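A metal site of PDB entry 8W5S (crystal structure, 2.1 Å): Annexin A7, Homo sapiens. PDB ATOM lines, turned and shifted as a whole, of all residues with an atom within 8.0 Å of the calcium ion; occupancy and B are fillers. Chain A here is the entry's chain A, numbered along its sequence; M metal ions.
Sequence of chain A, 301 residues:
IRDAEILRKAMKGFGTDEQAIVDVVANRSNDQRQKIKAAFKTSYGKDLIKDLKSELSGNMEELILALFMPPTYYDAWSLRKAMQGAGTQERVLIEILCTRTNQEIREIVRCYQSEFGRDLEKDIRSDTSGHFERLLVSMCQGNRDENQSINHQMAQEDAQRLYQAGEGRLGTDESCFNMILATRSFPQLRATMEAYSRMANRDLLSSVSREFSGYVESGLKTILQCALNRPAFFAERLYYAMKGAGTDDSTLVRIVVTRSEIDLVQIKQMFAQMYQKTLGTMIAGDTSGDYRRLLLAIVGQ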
ATOM      1  N   LYS A  50       3.865  14.080   1.368  1.00  0.00           N
ATOM      2  CA  LYS A  50       4.138  15.165   2.300  1.00  0.00           C
ATOM      3  C   LYS A  50       5.514  15.778   2.047  1.00  0.00           C
ATOM      4  O   LYS A  50       5.668  17.001   2.091  1.00  0.00           O
ATOM      5  CB  LYS A  50       4.021  14.669   3.737  1.00  0.00           C
ATOM      6  CG  LYS A  50       2.586  14.602   4.251  1.00  0.00           C
ATOM      7  CD  LYS A  50       1.926  15.976   4.228  1.00  0.00           C
ATOM      8  CE  LYS A  50       0.414  15.878   4.116  1.00  0.00           C
ATOM      9  NZ  LYS A  50      -0.019  14.965   3.035  1.00  0.00           N
ATOM     10  N   ASP A  51       6.524  14.946   1.796  1.00  0.00           N
ATOM     11  CA  ASP A  51       7.842  15.466   1.443  1.00  0.00           C
ATOM     12  C   ASP A  51       7.792  16.254   0.133  1.00  0.00           C
ATOM     13  O   ASP A  51       8.545  17.213  -0.030  1.00  0.00           O
ATOM     14  CB  ASP A  51       8.836  14.316   1.333  1.00  0.00           C
ATOM     15  CG  ASP A  51       9.523  14.013   2.645  1.00  0.00           C
ATOM     16  OD1 ASP A  51       9.389  14.823   3.593  1.00  0.00           O
ATOM     17  OD2 ASP A  51      10.180  12.958   2.748  1.00  0.00           O
ATOM     18  N   LEU A  52       6.911  15.850  -0.794  1.00  0.00           N
ATOM     19  CA  LEU A  52       6.748  16.608  -2.029  1.00  0.00           C
ATOM     20  C   LEU A  52       6.035  17.926  -1.796  1.00  0.00           C
ATOM     21  O   LEU A  52       6.319  18.922  -2.461  1.00  0.00           O
ATOM     22  CB  LEU A  52       5.999  15.772  -3.058  1.00  0.00           C
ATOM     23  CG  LEU A  52       6.785  14.684  -3.799  1.00  0.00           C
ATOM     24  CD1 LEU A  52       5.849  13.801  -4.600  1.00  0.00           C
ATOM     25  CD2 LEU A  52       7.845  15.307  -4.701  1.00  0.00           C
ATOM     26  N   LYS A  53       5.090  17.951  -0.844  1.00  0.00           N
ATOM     27  CA  LYS A  53       4.405  19.200  -0.534  1.00  0.00           C
ATOM     28  C   LYS A  53       5.334  20.206   0.135  1.00  0.00           C
ATOM     29  O   LYS A  53       5.112  21.411   0.030  1.00  0.00           O
ATOM     30  CB  LYS A  53       3.187  18.924   0.362  1.00  0.00           C
ATOM     31  CG  LYS A  53       1.886  18.684  -0.398  1.00  0.00           C
ATOM     32  CD  LYS A  53       0.878  17.931   0.448  1.00  0.00           C
ATOM     33  CE  LYS A  53      -0.452  18.654   0.472  1.00  0.00           C
ATOM     34  NZ  LYS A  53      -1.442  17.998   1.381  1.00  0.00           N
ATOM     35  N   SER A  54       6.378  19.718   0.809  1.00  0.00           N
ATOM     36  CA  SER A  54       7.292  20.620   1.495  1.00  0.00           C
ATOM     37  C   SER A  54       8.313  21.229   0.559  1.00  0.00           C
ATOM     38  O   SER A  54       8.792  22.343   0.814  1.00  0.00           O
ATOM     39  CB  SER A  54       8.005  19.871   2.625  1.00  0.00           C
ATOM     40  OG  SER A  54       8.537  18.642   2.166  1.00  0.00           O
ATOM     41  N   GLU A  55       8.662  20.544  -0.531  1.00  0.00           N
ATOM     42  CA  GLU A  55       9.728  20.987  -1.424  1.00  0.00           C
ATOM     43  C   GLU A  55       9.219  21.421  -2.800  1.00  0.00           C
ATOM     44  O   GLU A  55      10.023  21.849  -3.630  1.00  0.00           O
ATOM     45  CB  GLU A  55      10.787  19.892  -1.567  1.00  0.00           C
ATOM     46  CG  GLU A  55      11.832  19.916  -0.471  1.00  0.00           C
ATOM     47  CD  GLU A  55      13.251  19.822  -1.004  1.00  0.00           C
ATOM     48  OE1 GLU A  55      13.406  19.436  -2.174  1.00  0.00           O
ATOM     49  OE2 GLU A  55      14.188  20.145  -0.250  1.00  0.00           O
ATOM     50  N   LEU A  56       7.913  21.312  -3.063  1.00  0.00           N
ATOM     51  CA  LEU A  56       7.298  21.876  -4.250  1.00  0.00           C
ATOM     52  C   LEU A  56       6.320  22.972  -3.824  1.00  0.00           C
ATOM     53  O   LEU A  56       6.100  23.203  -2.629  1.00  0.00           O
ATOM     54  CB  LEU A  56       6.586  20.794  -5.077  1.00  0.00           C
ATOM     55  CG  LEU A  56       7.416  19.650  -5.645  1.00  0.00           C
ATOM     56  CD1 LEU A  56       6.502  18.636  -6.330  1.00  0.00           C
ATOM     57  CD2 LEU A  56       8.466  20.163  -6.624  1.00  0.00           C
ATOM     58  N   SER A  57       5.735  23.653  -4.801  1.00  0.00           N
ATOM     59  CA  SER A  57       4.832  24.758  -4.505  1.00  0.00           C
ATOM     60  C   SER A  57       4.060  25.137  -5.755  1.00  0.00           C
ATOM     61  O   SER A  57       4.481  24.862  -6.885  1.00  0.00           O
ATOM     62  CB  SER A  57       5.597  25.979  -3.967  1.00  0.00           C
ATOM     63  OG  SER A  57       6.654  26.341  -4.847  1.00  0.00           O
ATOM     64  N   GLY A  58       2.896  25.758  -5.542  1.00  0.00           N
ATOM     65  CA  GLY A  58       2.160  26.369  -6.642  1.00  0.00           C
ATOM     66  C   GLY A  58       1.568  25.341  -7.592  1.00  0.00           C
ATOM     67  O   GLY A  58       1.161  24.244  -7.181  1.00  0.00           O
ATOM     68  N   GLU A  61       3.230  21.958  -7.591  1.00  0.00           N
ATOM     69  CA  GLU A  61       2.839  21.081  -6.496  1.00  0.00           C
ATOM     70  C   GLU A  61       1.506  20.388  -6.782  1.00  0.00           C
ATOM     71  O   GLU A  61       1.383  19.172  -6.658  1.00  0.00           O
ATOM     72  CB  GLU A  61       2.766  21.875  -5.201  1.00  0.00           C
ATOM     73  CG  GLU A  61       2.831  21.036  -3.938  1.00  0.00           C
ATOM     74  CD  GLU A  61       2.545  21.846  -2.688  1.00  0.00           C
ATOM     75  OE1 GLU A  61       3.426  22.631  -2.270  1.00  0.00           O
ATOM     76  OE2 GLU A  61       1.444  21.698  -2.127  1.00  0.00           O
HETATM   77 CA    CA M   1       4.507  23.636  -0.533  1.00  0.00          CA
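Within 4 Å of the calcium ion: Lys 53, Leu 56 and Glu 61.
The nearest printed residue that does not touch the calcium ion is Ser 57 (4.1 Å).
The calcium ion is bound by OE1 of Glu 61 (2.3 Å), O of Lys 53 (2.4 Å) and O of Leu 56 (2.7 Å).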
